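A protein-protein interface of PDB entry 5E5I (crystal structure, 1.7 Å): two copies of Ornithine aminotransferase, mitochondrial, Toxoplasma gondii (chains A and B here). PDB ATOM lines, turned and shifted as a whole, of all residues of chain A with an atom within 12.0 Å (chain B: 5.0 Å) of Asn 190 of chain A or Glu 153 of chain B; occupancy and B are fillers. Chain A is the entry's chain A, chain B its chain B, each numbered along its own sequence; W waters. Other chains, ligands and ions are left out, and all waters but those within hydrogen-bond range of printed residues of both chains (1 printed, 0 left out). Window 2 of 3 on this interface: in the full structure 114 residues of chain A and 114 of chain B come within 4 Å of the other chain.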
ATOM      1  N   CYS A  46      -6.818  -0.484 -25.908  1.00  0.00           N
ATOM      2  CA  CYS A  46      -6.948   0.975 -25.748  1.00  0.00           C
ATOM      3  C   CYS A  46      -7.885   1.464 -26.868  1.00  0.00           C
ATOM      4  O   CYS A  46      -7.645   1.150 -28.043  1.00  0.00           O
ATOM      5  CB  CYS A  46      -5.567   1.592 -25.840  1.00  0.00           C
ATOM      6  SG  CYS A  46      -5.580   3.362 -25.451  1.00  0.00           S
ATOM      7  N   GLN A  47      -8.902   2.261 -26.491  1.00  0.00           N
ATOM      8  CA  GLN A  47      -9.996   2.763 -27.392  1.00  0.00           C
ATOM      9  C   GLN A  47      -9.631   3.943 -28.284  1.00  0.00           C
ATOM     10  O   GLN A  47     -10.491   4.767 -28.612  1.00  0.00           O
ATOM     11  CB  GLN A  47     -11.233   3.193 -26.575  1.00  0.00           C
ATOM     12  CG  GLN A  47     -11.088   4.495 -25.770  1.00  0.00           C
ATOM     13  CD  GLN A  47     -12.417   4.991 -25.159  1.00  0.00           C
ATOM     14  OE1 GLN A  47     -13.491   4.565 -25.535  1.00  0.00           O
ATOM     15  NE2 GLN A  47     -12.324   5.874 -24.213  1.00  0.00           N
ATOM     16  N   ASN A  48      -8.391   3.982 -28.735  1.00  0.00           N
ATOM     17  CA  ASN A  48      -7.922   5.148 -29.524  1.00  0.00           C
ATOM     18  C   ASN A  48      -8.208   5.106 -31.029  1.00  0.00           C
ATOM     19  O   ASN A  48      -7.835   6.012 -31.752  1.00  0.00           O
ATOM     20  CB  ASN A  48      -6.479   5.498 -29.246  1.00  0.00           C
ATOM     21  CG  ASN A  48      -5.527   4.431 -29.646  1.00  0.00           C
ATOM     22  OD1 ASN A  48      -5.475   3.396 -29.014  1.00  0.00           O
ATOM     23  ND2 ASN A  48      -4.674   4.721 -30.616  1.00  0.00           N
ATOM     24  N   ARG A 174       2.704  10.770 -34.120  1.00  0.00           N
ATOM     25  CA  ARG A 174       1.978  10.933 -32.893  1.00  0.00           C
ATOM     26  C   ARG A 174       2.791  11.242 -31.624  1.00  0.00           C
ATOM     27  O   ARG A 174       2.253  11.174 -30.511  1.00  0.00           O
ATOM     28  CB  ARG A 174       1.125   9.675 -32.687  1.00  0.00           C
ATOM     29  CG  ARG A 174       0.074   9.514 -33.801  1.00  0.00           C
ATOM     30  CD  ARG A 174      -1.054  10.517 -33.632  1.00  0.00           C
ATOM     31  NE  ARG A 174      -2.181  10.271 -34.539  1.00  0.00           N
ATOM     32  CZ  ARG A 174      -3.418  10.709 -34.380  1.00  0.00           C
ATOM     33  NH1 ARG A 174      -3.764  11.473 -33.329  1.00  0.00           N
ATOM     34  NH2 ARG A 174      -4.348  10.346 -35.262  1.00  0.00           N
ATOM     35  N   THR A 175       4.065  11.547 -31.781  1.00  0.00           N
ATOM     36  CA  THR A 175       4.876  11.876 -30.652  1.00  0.00           C
ATOM     37  C   THR A 175       4.441  13.267 -30.203  1.00  0.00           C
ATOM     38  O   THR A 175       3.759  13.963 -30.932  1.00  0.00           O
ATOM     39  CB  THR A 175       6.360  11.962 -31.017  1.00  0.00           C
ATOM     40  OG1 THR A 175       6.526  12.908 -32.072  1.00  0.00           O
ATOM     41  CG2 THR A 175       6.927  10.609 -31.476  1.00  0.00           C
ATOM     42  N   ILE A 176       4.859  13.653 -29.010  1.00  0.00           N
ATOM     43  CA  ILE A 176       4.515  15.022 -28.508  1.00  0.00           C
ATOM     44  C   ILE A 176       5.031  16.103 -29.465  1.00  0.00           C
ATOM     45  O   ILE A 176       4.328  17.112 -29.723  1.00  0.00           O
ATOM     46  CB  ILE A 176       4.918  15.187 -27.040  1.00  0.00           C
ATOM     47  CG1 ILE A 176       4.015  14.287 -26.175  1.00  0.00           C
ATOM     48  CG2 ILE A 176       4.889  16.682 -26.584  1.00  0.00           C
ATOM     49  CD1 ILE A 176       4.450  14.128 -24.736  1.00  0.00           C
ATOM     50  N   THR A 177       6.221  15.914 -30.009  1.00  0.00           N
ATOM     51  CA  THR A 177       6.749  16.864 -30.930  1.00  0.00           C
ATOM     52  C   THR A 177       5.927  16.944 -32.206  1.00  0.00           C
ATOM     53  O   THR A 177       5.710  18.046 -32.746  1.00  0.00           O
ATOM     54  CB  THR A 177       8.253  16.707 -31.098  1.00  0.00           C
ATOM     55  OG1 THR A 177       8.877  16.918 -29.819  1.00  0.00           O
ATOM     56  CG2 THR A 177       8.807  17.669 -32.020  1.00  0.00           C
ATOM     57  N   ALA A 178       5.369  15.821 -32.646  1.00  0.00           N
ATOM     58  CA  ALA A 178       4.511  15.845 -33.813  1.00  0.00           C
ATOM     59  C   ALA A 178       3.208  16.525 -33.468  1.00  0.00           C
ATOM     60  O   ALA A 178       2.775  17.406 -34.203  1.00  0.00           O
ATOM     61  CB  ALA A 178       4.285  14.442 -34.351  1.00  0.00           C
ATOM     62  N   CYS A 179       2.627  16.241 -32.308  1.00  0.00           N
ATOM     63  CA  CYS A 179       1.382  16.906 -31.916  1.00  0.00           C
ATOM     64  C   CYS A 179       1.610  18.403 -31.818  1.00  0.00           C
ATOM     65  O   CYS A 179       0.721  19.180 -32.143  1.00  0.00           O
ATOM     66  CB  CYS A 179       0.875  16.456 -30.551  1.00  0.00           C
ATOM     67  SG  CYS A 179       0.559  14.665 -30.501  1.00  0.00           S
ATOM     68  N   SER A 180       2.803  18.792 -31.364  1.00  0.00           N
ATOM     69  CA  SER A 180       3.167  20.243 -31.163  1.00  0.00           C
ATOM     70  C   SER A 180       3.262  21.008 -32.488  1.00  0.00           C
ATOM     71  O   SER A 180       3.251  22.245 -32.492  1.00  0.00           O
ATOM     72  CB  SER A 180       4.536  20.307 -30.493  1.00  0.00           C
ATOM     73  OG  SER A 180       4.560  19.667 -29.256  1.00  0.00           O
ATOM     74  N   SER A 181       3.377  20.259 -33.599  1.00  0.00           N
ATOM     75  CA  SER A 181       3.482  20.803 -34.950  1.00  0.00           C
ATOM     76  C   SER A 181       2.301  20.506 -35.897  1.00  0.00           C
ATOM     77  O   SER A 181       2.410  20.732 -37.089  1.00  0.00           O
ATOM     78  CB  SER A 181       4.835  20.418 -35.572  1.00  0.00           C
ATOM     79  OG  SER A 181       5.027  18.987 -35.712  1.00  0.00           O
ATOM     80  N   SER A 182       1.190  20.008 -35.336  1.00  0.00           N
ATOM     81  CA  SER A 182      -0.049  19.664 -36.066  1.00  0.00           C
ATOM     82  C   SER A 182      -1.071  20.809 -35.909  1.00  0.00           C
ATOM     83  O   SER A 182      -0.986  21.608 -34.965  1.00  0.00           O
ATOM     84  CB  SER A 182      -0.684  18.397 -35.467  1.00  0.00           C
ATOM     85  OG  SER A 182      -1.912  17.991 -36.078  1.00  0.00           O
ATOM     86  N   THR A 183      -1.992  20.896 -36.868  1.00  0.00           N
ATOM     87  CA  THR A 183      -3.108  21.882 -36.825  1.00  0.00           C
ATOM     88  C   THR A 183      -4.382  21.089 -36.717  1.00  0.00           C
ATOM     89  O   THR A 183      -5.478  21.652 -36.787  1.00  0.00           O
ATOM     90  CB  THR A 183      -3.174  22.809 -38.067  1.00  0.00           C
ATOM     91  OG1 THR A 183      -3.368  22.024 -39.268  1.00  0.00           O
ATOM     92  CG2 THR A 183      -1.885  23.598 -38.168  1.00  0.00           C
ATOM     93  N   THR A 184      -4.259  19.756 -36.583  1.00  0.00           N
ATOM     94  CA  THR A 184      -5.440  18.949 -36.404  1.00  0.00           C
ATOM     95  C   THR A 184      -5.830  18.834 -34.900  1.00  0.00           C
ATOM     96  O   THR A 184      -5.133  18.168 -34.132  1.00  0.00           O
ATOM     97  CB  THR A 184      -5.169  17.549 -36.931  1.00  0.00           C
ATOM     98  OG1 THR A 184      -4.613  17.674 -38.234  1.00  0.00           O
ATOM     99  CG2 THR A 184      -6.505  16.757 -36.965  1.00  0.00           C
ATOM    100  N   PHE A 185      -6.964  19.411 -34.518  1.00  0.00           N
ATOM    101  CA  PHE A 185      -7.438  19.487 -33.121  1.00  0.00           C
ATOM    102  C   PHE A 185      -7.271  18.192 -32.324  1.00  0.00           C
ATOM    103  O   PHE A 185      -6.618  18.184 -31.308  1.00  0.00           O
ATOM    104  CB  PHE A 185      -8.893  19.969 -33.065  1.00  0.00           C
ATOM    105  CG  PHE A 185      -9.405  20.171 -31.673  1.00  0.00           C
ATOM    106  CD1 PHE A 185      -9.085  21.337 -30.963  1.00  0.00           C
ATOM    107  CD2 PHE A 185     -10.214  19.219 -31.063  1.00  0.00           C
ATOM    108  CE1 PHE A 185      -9.527  21.506 -29.655  1.00  0.00           C
ATOM    109  CE2 PHE A 185     -10.666  19.389 -29.789  1.00  0.00           C
ATOM    110  CZ  PHE A 185     -10.328  20.528 -29.066  1.00  0.00           C
ATOM    111  N   ASP A 186      -7.794  17.080 -32.826  1.00  0.00           N
ATOM    112  CA  ASP A 186      -7.659  15.836 -32.075  1.00  0.00           C
ATOM    113  C   ASP A 186      -6.222  15.349 -31.882  1.00  0.00           C
ATOM    114  O   ASP A 186      -5.946  14.620 -30.922  1.00  0.00           O
ATOM    115  CB  ASP A 186      -8.516  14.708 -32.674  1.00  0.00           C
ATOM    116  CG  ASP A 186     -10.003  14.854 -32.353  1.00  0.00           C
ATOM    117  OD1 ASP A 186     -10.389  15.549 -31.369  1.00  0.00           O
ATOM    118  OD2 ASP A 186     -10.780  14.201 -33.081  1.00  0.00           O
ATOM    119  N   CYS A 187      -5.309  15.736 -32.766  1.00  0.00           N
ATOM    120  CA  CYS A 187      -3.912  15.341 -32.615  1.00  0.00           C
ATOM    121  C   CYS A 187      -3.200  16.039 -31.470  1.00  0.00           C
ATOM    122  O   CYS A 187      -2.392  15.426 -30.804  1.00  0.00           O
ATOM    123  CB  CYS A 187      -3.114  15.600 -33.892  1.00  0.00           C
ATOM    124  SG  CYS A 187      -3.477  14.422 -35.202  1.00  0.00           S
ATOM    125  N   TYR A 188      -3.497  17.318 -31.240  1.00  0.00           N
ATOM    126  CA  TYR A 188      -2.805  18.067 -30.194  1.00  0.00           C
ATOM    127  C   TYR A 188      -3.570  18.394 -28.905  1.00  0.00           C
ATOM    128  O   TYR A 188      -2.963  18.622 -27.858  1.00  0.00           O
ATOM    129  CB  TYR A 188      -2.258  19.384 -30.792  1.00  0.00           C
ATOM    130  CG  TYR A 188      -3.319  20.372 -31.222  1.00  0.00           C
ATOM    131  CD1 TYR A 188      -3.965  21.173 -30.261  1.00  0.00           C
ATOM    132  CD2 TYR A 188      -3.625  20.591 -32.579  1.00  0.00           C
ATOM    133  CE1 TYR A 188      -4.926  22.117 -30.623  1.00  0.00           C
ATOM    134  CE2 TYR A 188      -4.581  21.558 -32.955  1.00  0.00           C
ATOM    135  CZ  TYR A 188      -5.218  22.301 -31.979  1.00  0.00           C
ATOM    136  OH  TYR A 188      -6.180  23.231 -32.299  1.00  0.00           O
ATOM    137  N   ASN A 189      -4.896  18.422 -28.961  1.00  0.00           N
ATOM    138  CA  ASN A 189      -5.701  18.844 -27.819  1.00  0.00           C
ATOM    139  C   ASN A 189      -5.373  18.091 -26.545  1.00  0.00           C
ATOM    140  O   ASN A 189      -5.408  16.856 -26.522  1.00  0.00           O
ATOM    141  CB  ASN A 189      -7.194  18.662 -28.137  1.00  0.00           C
ATOM    142  CG  ASN A 189      -8.077  19.117 -27.004  1.00  0.00           C
ATOM    143  OD1 ASN A 189      -7.958  20.239 -26.526  1.00  0.00           O
ATOM    144  ND2 ASN A 189      -8.998  18.267 -26.603  1.00  0.00           N
ATOM    145  N   ASN A 190      -5.086  18.838 -25.488  1.00  0.00           N
ATOM    146  CA  ASN A 190      -4.773  18.282 -24.155  1.00  0.00           C
ATOM    147  C   ASN A 190      -3.511  17.403 -24.057  1.00  0.00           C
ATOM    148  O   ASN A 190      -3.393  16.582 -23.179  1.00  0.00           O
ATOM    149  CB  ASN A 190      -5.999  17.620 -23.537  1.00  0.00           C
ATOM    150  CG  ASN A 190      -6.999  18.633 -22.981  1.00  0.00           C
ATOM    151  OD1 ASN A 190      -6.665  19.776 -22.745  1.00  0.00           O
ATOM    152  ND2 ASN A 190      -8.224  18.202 -22.783  1.00  0.00           N
ATOM    153  N   PHE A 191      -2.591  17.581 -24.994  1.00  0.00           N
ATOM    154  CA  PHE A 191      -1.307  16.904 -24.954  1.00  0.00           C
ATOM    155  C   PHE A 191      -0.116  17.833 -24.658  1.00  0.00           C
ATOM    156  O   PHE A 191       1.044  17.408 -24.640  1.00  0.00           O
ATOM    157  CB  PHE A 191      -1.053  16.084 -26.223  1.00  0.00           C
ATOM    158  CG  PHE A 191      -2.043  14.976 -26.455  1.00  0.00           C
ATOM    159  CD1 PHE A 191      -2.226  13.973 -25.519  1.00  0.00           C
ATOM    160  CD2 PHE A 191      -2.711  14.866 -27.656  1.00  0.00           C
ATOM    161  CE1 PHE A 191      -3.106  12.914 -25.756  1.00  0.00           C
ATOM    162  CE2 PHE A 191      -3.604  13.831 -27.886  1.00  0.00           C
ATOM    163  CZ  PHE A 191      -3.775  12.845 -26.953  1.00  0.00           C
ATOM    164  N   GLY A 192      -0.383  19.112 -24.402  1.00  0.00           N
ATOM    165  CA  GLY A 192       0.722  20.037 -24.119  1.00  0.00           C
ATOM    166  C   GLY A 192       1.257  19.980 -22.689  1.00  0.00           C
ATOM    167  O   GLY A 192       0.751  19.250 -21.891  1.00  0.00           O
ATOM    168  N   PRO A 193       2.197  20.844 -22.312  1.00  0.00           N
ATOM    169  CA  PRO A 193       2.737  21.912 -23.158  1.00  0.00           C
ATOM    170  C   PRO A 193       3.543  21.416 -24.342  1.00  0.00           C
ATOM    171  O   PRO A 193       4.087  20.277 -24.362  1.00  0.00           O
ATOM    172  CB  PRO A 193       3.570  22.746 -22.176  1.00  0.00           C
ATOM    173  CG  PRO A 193       4.000  21.737 -21.148  1.00  0.00           C
ATOM    174  CD  PRO A 193       2.795  20.863 -20.967  1.00  0.00           C
ATOM    175  N   PHE A 194       3.593  22.253 -25.354  1.00  0.00           N
ATOM    176  CA  PHE A 194       4.200  21.815 -26.600  1.00  0.00           C
ATOM    177  C   PHE A 194       5.628  22.210 -26.843  1.00  0.00           C
ATOM    178  O   PHE A 194       6.123  23.227 -26.331  1.00  0.00           O
ATOM    179  CB  PHE A 194       3.299  22.268 -27.766  1.00  0.00           C
ATOM    180  CG  PHE A 194       1.867  21.843 -27.604  1.00  0.00           C
ATOM    181  CD1 PHE A 194       1.486  20.499 -27.815  1.00  0.00           C
ATOM    182  CD2 PHE A 194       0.888  22.752 -27.223  1.00  0.00           C
ATOM    183  CE1 PHE A 194       0.147  20.136 -27.650  1.00  0.00           C
ATOM    184  CE2 PHE A 194      -0.447  22.380 -27.047  1.00  0.00           C
ATOM    185  CZ  PHE A 194      -0.811  21.065 -27.270  1.00  0.00           C
ATOM    186  N   THR A 195       6.290  21.389 -27.648  1.00  0.00           N
ATOM    187  CA  THR A 195       7.646  21.647 -28.120  1.00  0.00           C
ATOM    188  C   THR A 195       7.636  22.948 -28.980  1.00  0.00           C
ATOM    189  O   THR A 195       6.871  23.047 -29.928  1.00  0.00           O
ATOM    190  CB  THR A 195       8.112  20.521 -29.023  1.00  0.00           C
ATOM    191  OG1 THR A 195       7.933  19.260 -28.340  1.00  0.00           O
ATOM    192  CG2 THR A 195       9.533  20.696 -29.391  1.00  0.00           C
ATOM    193  N   LYS B 145       1.553  11.464 -23.010  1.00  0.00           N
ATOM    194  CA  LYS B 145       0.309  11.979 -23.605  1.00  0.00           C
ATOM    195  C   LYS B 145      -0.929  11.579 -22.741  1.00  0.00           C
ATOM    196  O   LYS B 145      -1.794  12.385 -22.445  1.00  0.00           O
ATOM    197  CB  LYS B 145       0.165  11.506 -25.047  1.00  0.00           C
ATOM    198  CG  LYS B 145       1.208  12.105 -25.998  1.00  0.00           C
ATOM    199  CD  LYS B 145       1.087  11.550 -27.414  1.00  0.00           C
ATOM    200  CE  LYS B 145      -0.213  11.926 -28.065  1.00  0.00           C
ATOM    201  NZ  LYS B 145      -0.279  11.474 -29.449  1.00  0.00           N
ATOM    202  N   ARG B 148      -0.856  13.397 -19.426  1.00  0.00           N
ATOM    203  CA  ARG B 148      -1.223  14.811 -19.565  1.00  0.00           C
ATOM    204  C   ARG B 148      -2.730  15.013 -19.831  1.00  0.00           C
ATOM    205  O   ARG B 148      -3.363  15.858 -19.202  1.00  0.00           O
ATOM    206  CB  ARG B 148      -0.412  15.489 -20.674  1.00  0.00           C
ATOM    207  CG  ARG B 148       1.080  15.599 -20.357  1.00  0.00           C
ATOM    208  CD  ARG B 148       1.847  16.044 -21.601  1.00  0.00           C
ATOM    209  NE  ARG B 148       3.120  16.664 -21.258  1.00  0.00           N
ATOM    210  CZ  ARG B 148       3.857  17.446 -22.078  1.00  0.00           C
ATOM    211  NH1 ARG B 148       3.451  17.756 -23.325  1.00  0.00           N
ATOM    212  NH2 ARG B 148       5.005  17.960 -21.643  1.00  0.00           N
ATOM    213  N   LYS B 149      -3.285  14.262 -20.788  1.00  0.00           N
ATOM    214  CA  LYS B 149      -4.702  14.362 -21.164  1.00  0.00           C
ATOM    215  C   LYS B 149      -5.582  13.982 -19.928  1.00  0.00           C
ATOM    216  O   LYS B 149      -6.580  14.659 -19.634  1.00  0.00           O
ATOM    217  CB  LYS B 149      -4.981  13.549 -22.426  1.00  0.00           C
ATOM    218  CG  LYS B 149      -6.293  13.847 -23.080  1.00  0.00           C
ATOM    219  CD  LYS B 149      -6.410  13.326 -24.481  1.00  0.00           C
ATOM    220  CE  LYS B 149      -7.678  13.780 -25.171  1.00  0.00           C
ATOM    221  NZ  LYS B 149      -8.940  13.188 -24.659  1.00  0.00           N
ATOM    222  N   TRP B 150      -5.129  12.983 -19.171  1.00  0.00           N
ATOM    223  CA  TRP B 150      -5.821  12.557 -17.923  1.00  0.00           C
ATOM    224  C   TRP B 150      -5.764  13.708 -16.903  1.00  0.00           C
ATOM    225  O   TRP B 150      -6.745  14.019 -16.245  1.00  0.00           O
ATOM    226  CB  TRP B 150      -5.184  11.268 -17.347  1.00  0.00           C
ATOM    227  CG  TRP B 150      -5.723  10.905 -15.992  1.00  0.00           C
ATOM    228  CD1 TRP B 150      -6.850  10.197 -15.720  1.00  0.00           C
ATOM    229  CD2 TRP B 150      -5.142  11.226 -14.745  1.00  0.00           C
ATOM    230  NE1 TRP B 150      -7.033  10.104 -14.370  1.00  0.00           N
ATOM    231  CE2 TRP B 150      -5.975  10.705 -13.744  1.00  0.00           C
ATOM    232  CE3 TRP B 150      -4.000  11.919 -14.368  1.00  0.00           C
ATOM    233  CZ2 TRP B 150      -5.702  10.865 -12.382  1.00  0.00           C
ATOM    234  CZ3 TRP B 150      -3.725  12.080 -13.002  1.00  0.00           C
ATOM    235  CH2 TRP B 150      -4.576  11.544 -12.029  1.00  0.00           C
ATOM    236  N   ALA B 151      -4.600  14.349 -16.793  1.00  0.00           N
ATOM    237  CA  ALA B 151      -4.477  15.466 -15.840  1.00  0.00           C
ATOM    238  C   ALA B 151      -5.416  16.596 -16.148  1.00  0.00           C
ATOM    239  O   ALA B 151      -6.001  17.180 -15.238  1.00  0.00           O
ATOM    240  CB  ALA B 151      -3.059  15.980 -15.792  1.00  0.00           C
ATOM    241  N   TYR B 152      -5.535  16.927 -17.411  1.00  0.00           N
ATOM    242  CA  TYR B 152      -6.425  17.992 -17.842  1.00  0.00           C
ATOM    243  C   TYR B 152      -7.907  17.659 -17.745  1.00  0.00           C
ATOM    244  O   TYR B 152      -8.682  18.527 -17.378  1.00  0.00           O
ATOM    245  CB  TYR B 152      -6.098  18.411 -19.284  1.00  0.00           C
ATOM    246  CG  TYR B 152      -4.670  18.905 -19.434  1.00  0.00           C
ATOM    247  CD1 TYR B 152      -4.184  19.928 -18.615  1.00  0.00           C
ATOM    248  CD2 TYR B 152      -3.845  18.449 -20.437  1.00  0.00           C
ATOM    249  CE1 TYR B 152      -2.896  20.382 -18.735  1.00  0.00           C
ATOM    250  CE2 TYR B 152      -2.542  18.889 -20.560  1.00  0.00           C
ATOM    251  CZ  TYR B 152      -2.089  19.879 -19.710  1.00  0.00           C
ATOM    252  OH  TYR B 152      -0.802  20.351 -19.834  1.00  0.00           O
ATOM    253  N   GLU B 153      -8.280  16.419 -18.072  1.00  0.00           N
ATOM    254  CA  GLU B 153      -9.680  15.986 -18.148  1.00  0.00           C
ATOM    255  C   GLU B 153     -10.234  15.474 -16.835  1.00  0.00           C
ATOM    256  O   GLU B 153     -11.367  15.797 -16.499  1.00  0.00           O
ATOM    257  CB  GLU B 153      -9.894  15.018 -19.345  1.00  0.00           C
ATOM    258  CG  GLU B 153      -9.601  15.705 -20.685  1.00  0.00           C
ATOM    259  CD  GLU B 153      -9.690  14.799 -21.913  1.00  0.00           C
ATOM    260  OE1 GLU B 153     -10.031  13.623 -21.739  1.00  0.00           O
ATOM    261  OE2 GLU B 153      -9.385  15.283 -23.035  1.00  0.00           O
ATOM    262  N   VAL B 154      -9.396  14.809 -16.038  1.00  0.00           N
ATOM    263  CA  VAL B 154      -9.824  14.187 -14.786  1.00  0.00           C
ATOM    264  C   VAL B 154      -9.367  14.972 -13.571  1.00  0.00           C
ATOM    265  O   VAL B 154     -10.171  15.225 -12.717  1.00  0.00           O
ATOM    266  CB  VAL B 154      -9.405  12.696 -14.721  1.00  0.00           C
ATOM    267  CG1 VAL B 154      -9.913  12.068 -13.429  1.00  0.00           C
ATOM    268  CG2 VAL B 154      -9.990  11.946 -15.888  1.00  0.00           C
ATOM    269  N   LYS B 155      -8.097  15.350 -13.451  1.00  0.00           N
ATOM    270  CA  LYS B 155      -7.694  16.217 -12.314  1.00  0.00           C
ATOM    271  C   LYS B 155      -8.098  17.667 -12.584  1.00  0.00           C
ATOM    272  O   LYS B 155      -8.012  18.502 -11.684  1.00  0.00           O
ATOM    273  CB  LYS B 155      -6.175  16.240 -12.070  1.00  0.00           C
ATOM    274  CG  LYS B 155      -5.565  14.983 -11.554  1.00  0.00           C
ATOM    275  CD  LYS B 155      -4.061  15.122 -11.292  1.00  0.00           C
ATOM    276  CE  LYS B 155      -3.710  15.911 -10.054  1.00  0.00           C
ATOM    277  NZ  LYS B 155      -2.289  15.690  -9.657  1.00  0.00           N
ATOM    278  N   GLU B 156      -8.472  17.992 -13.829  1.00  0.00           N
ATOM    279  CA  GLU B 156      -8.877  19.372 -14.195  1.00  0.00           C
ATOM    280  C   GLU B 156      -7.828  20.458 -13.899  1.00  0.00           C
ATOM    281  O   GLU B 156      -8.181  21.588 -13.541  1.00  0.00           O
ATOM    282  CB  GLU B 156     -10.183  19.774 -13.524  1.00  0.00           C
ATOM    283  CG  GLU B 156     -11.382  18.909 -13.830  1.00  0.00           C
ATOM    284  CD  GLU B 156     -12.568  19.304 -12.962  1.00  0.00           C
ATOM    285  OE1 GLU B 156     -12.783  20.529 -12.745  1.00  0.00           O
ATOM    286  OE2 GLU B 156     -13.274  18.392 -12.482  1.00  0.00           O
ATOM    287  N   VAL B 307      -8.935   8.026 -21.768  1.00  0.00           N
ATOM    288  CA  VAL B 307      -8.807   9.439 -22.240  1.00  0.00           C
ATOM    289  C   VAL B 307      -8.345   9.483 -23.711  1.00  0.00           C
ATOM    290  O   VAL B 307      -8.601  10.448 -24.430  1.00  0.00           O
ATOM    291  CB  VAL B 307      -7.858  10.280 -21.387  1.00  0.00           C
ATOM    292  CG1 VAL B 307      -8.290  10.251 -19.950  1.00  0.00           C
ATOM    293  CG2 VAL B 307      -6.410   9.840 -21.576  1.00  0.00           C
HETATM  294  O   HOH W   1      -2.243  12.780 -31.081  1.00  0.00           O
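No position is printed for both chains.
Water W1 lies within hydrogen-bond range of O of Cys 187 of chain A (2.7 Å), NZ of Lys 145 of chain B (2.9 Å), NH1 of Arg 174 of chain A (3.0 Å) and SG of Cys 179 of chain A (3.4 Å).
Hydrophobic or aromatic side chains of chain B within 4 Å of the printed part of chain A: Tyr 152. Along chain B the printed residues that touch a printed residue of chain A span positions 145 to 153. Among the printed residues, no Asp or Glu carboxylate lies within 4 Å of a Lys or Arg side-chain nitrogen of the other chain.
OG of Ser 180 of chain A is in hydrogen-bond range of O of Ile 176 of chain A (2.6 Å). NH1 of Arg 174 of chain A lies within hydrogen-bond range of SG of Cys 187 of chain A, 3.5 Å away. O of Val 307 of chain B lies within hydrogen-bond range of NZ of Lys 149 of chain B. The side-chain sulfur of Cys 179 of chain A sits at hydrogen-bond distance from the backbone carbonyl oxygen of Cys 187 of chain A, 3.1 Å away. The side-chain amino group (NZ) of Lys 149 of chain B is in salt-bridge range of the side-chain carboxylate (OE2) of Glu 153 of chain B (2.7 Å). The side-chain sulfur (SG) of Cys 179 of chain A sits at hydrogen-bond distance from the backbone carbonyl oxygen (O) of Thr 175 of chain A.
The side-chain amide nitrogen (ND2) of Asn 190 of chain A is in hydrogen-bond range of the side-chain carboxylate (OE2) of Glu 153 of chain B, at 3.2 Å. The backbone carbonyl oxygen of Phe 191 of chain A is in hydrogen-bond range of the guanidinium group of Arg 148 of chain B (2.8 Å). SG of Cys 179 of chain A lies within hydrogen-bond range of NZ of Lys 145 of chain B. The side-chain hydroxyl (OH) of Tyr 152 of chain B lies within hydrogen-bond range of the backbone carbonyl oxygen (O) of Gly 192 of chain A (2.8 Å). The backbone carbonyl oxygen of Gly 192 of chain A sits close to the guanidinium group of Arg 148 of chain B. O of Asn 190 of chain A sits close to N of Lys 149 of chain B, at 3.3 Å. O of Pro 193 of chain A is in hydrogen-bond range of NH1 of Arg 148 of chain B (2.8 Å). O of Arg 174 of chain A is in hydrogen-bond range of NZ of Lys 145 of chain B, 2.8 Å away.
Among the printed residues, merely in contact across the chains: Asn 190 of chain A with Tyr 152 of chain B, Phe 191 of chain A with Lys 145 of chain B, Ile 176 of chain A with Lys 145 of chain B, Phe 191 of chain A with Lys 149 of chain B, Ile 176 of chain A with Arg 148 of chain B, Asn 190 of chain A with Arg 148 of chain B and Pro 193 of chain A with Tyr 152 of chain B.
Of the printed residues of chain B, Asn 190 of chain A touches Arg 148, Lys 149, Tyr 152 and Glu 153. No residue of chain A comes within 4 Å of Ala 151 of chain B. Of the printed residues of chain A, Tyr 152 of chain B touches Asn 190 (3.3 Å), Gly 192 (2.8 Å) and Pro 193 (3.8 Å). No residue of chain A comes within 4 Å of Val 154 of chain B. Printed residues of chain B within 4 Å of Phe 191 of chain A: Lys 145, Arg 148 and Lys 149. Printed residues of chain B within 4 Å of Arg 174 of chain A: Lys 145 (2.8 Å). The nearest printed residue of chain B that does not touch Ile 176 of chain A is Lys 149 of chain B (8.7 Å).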
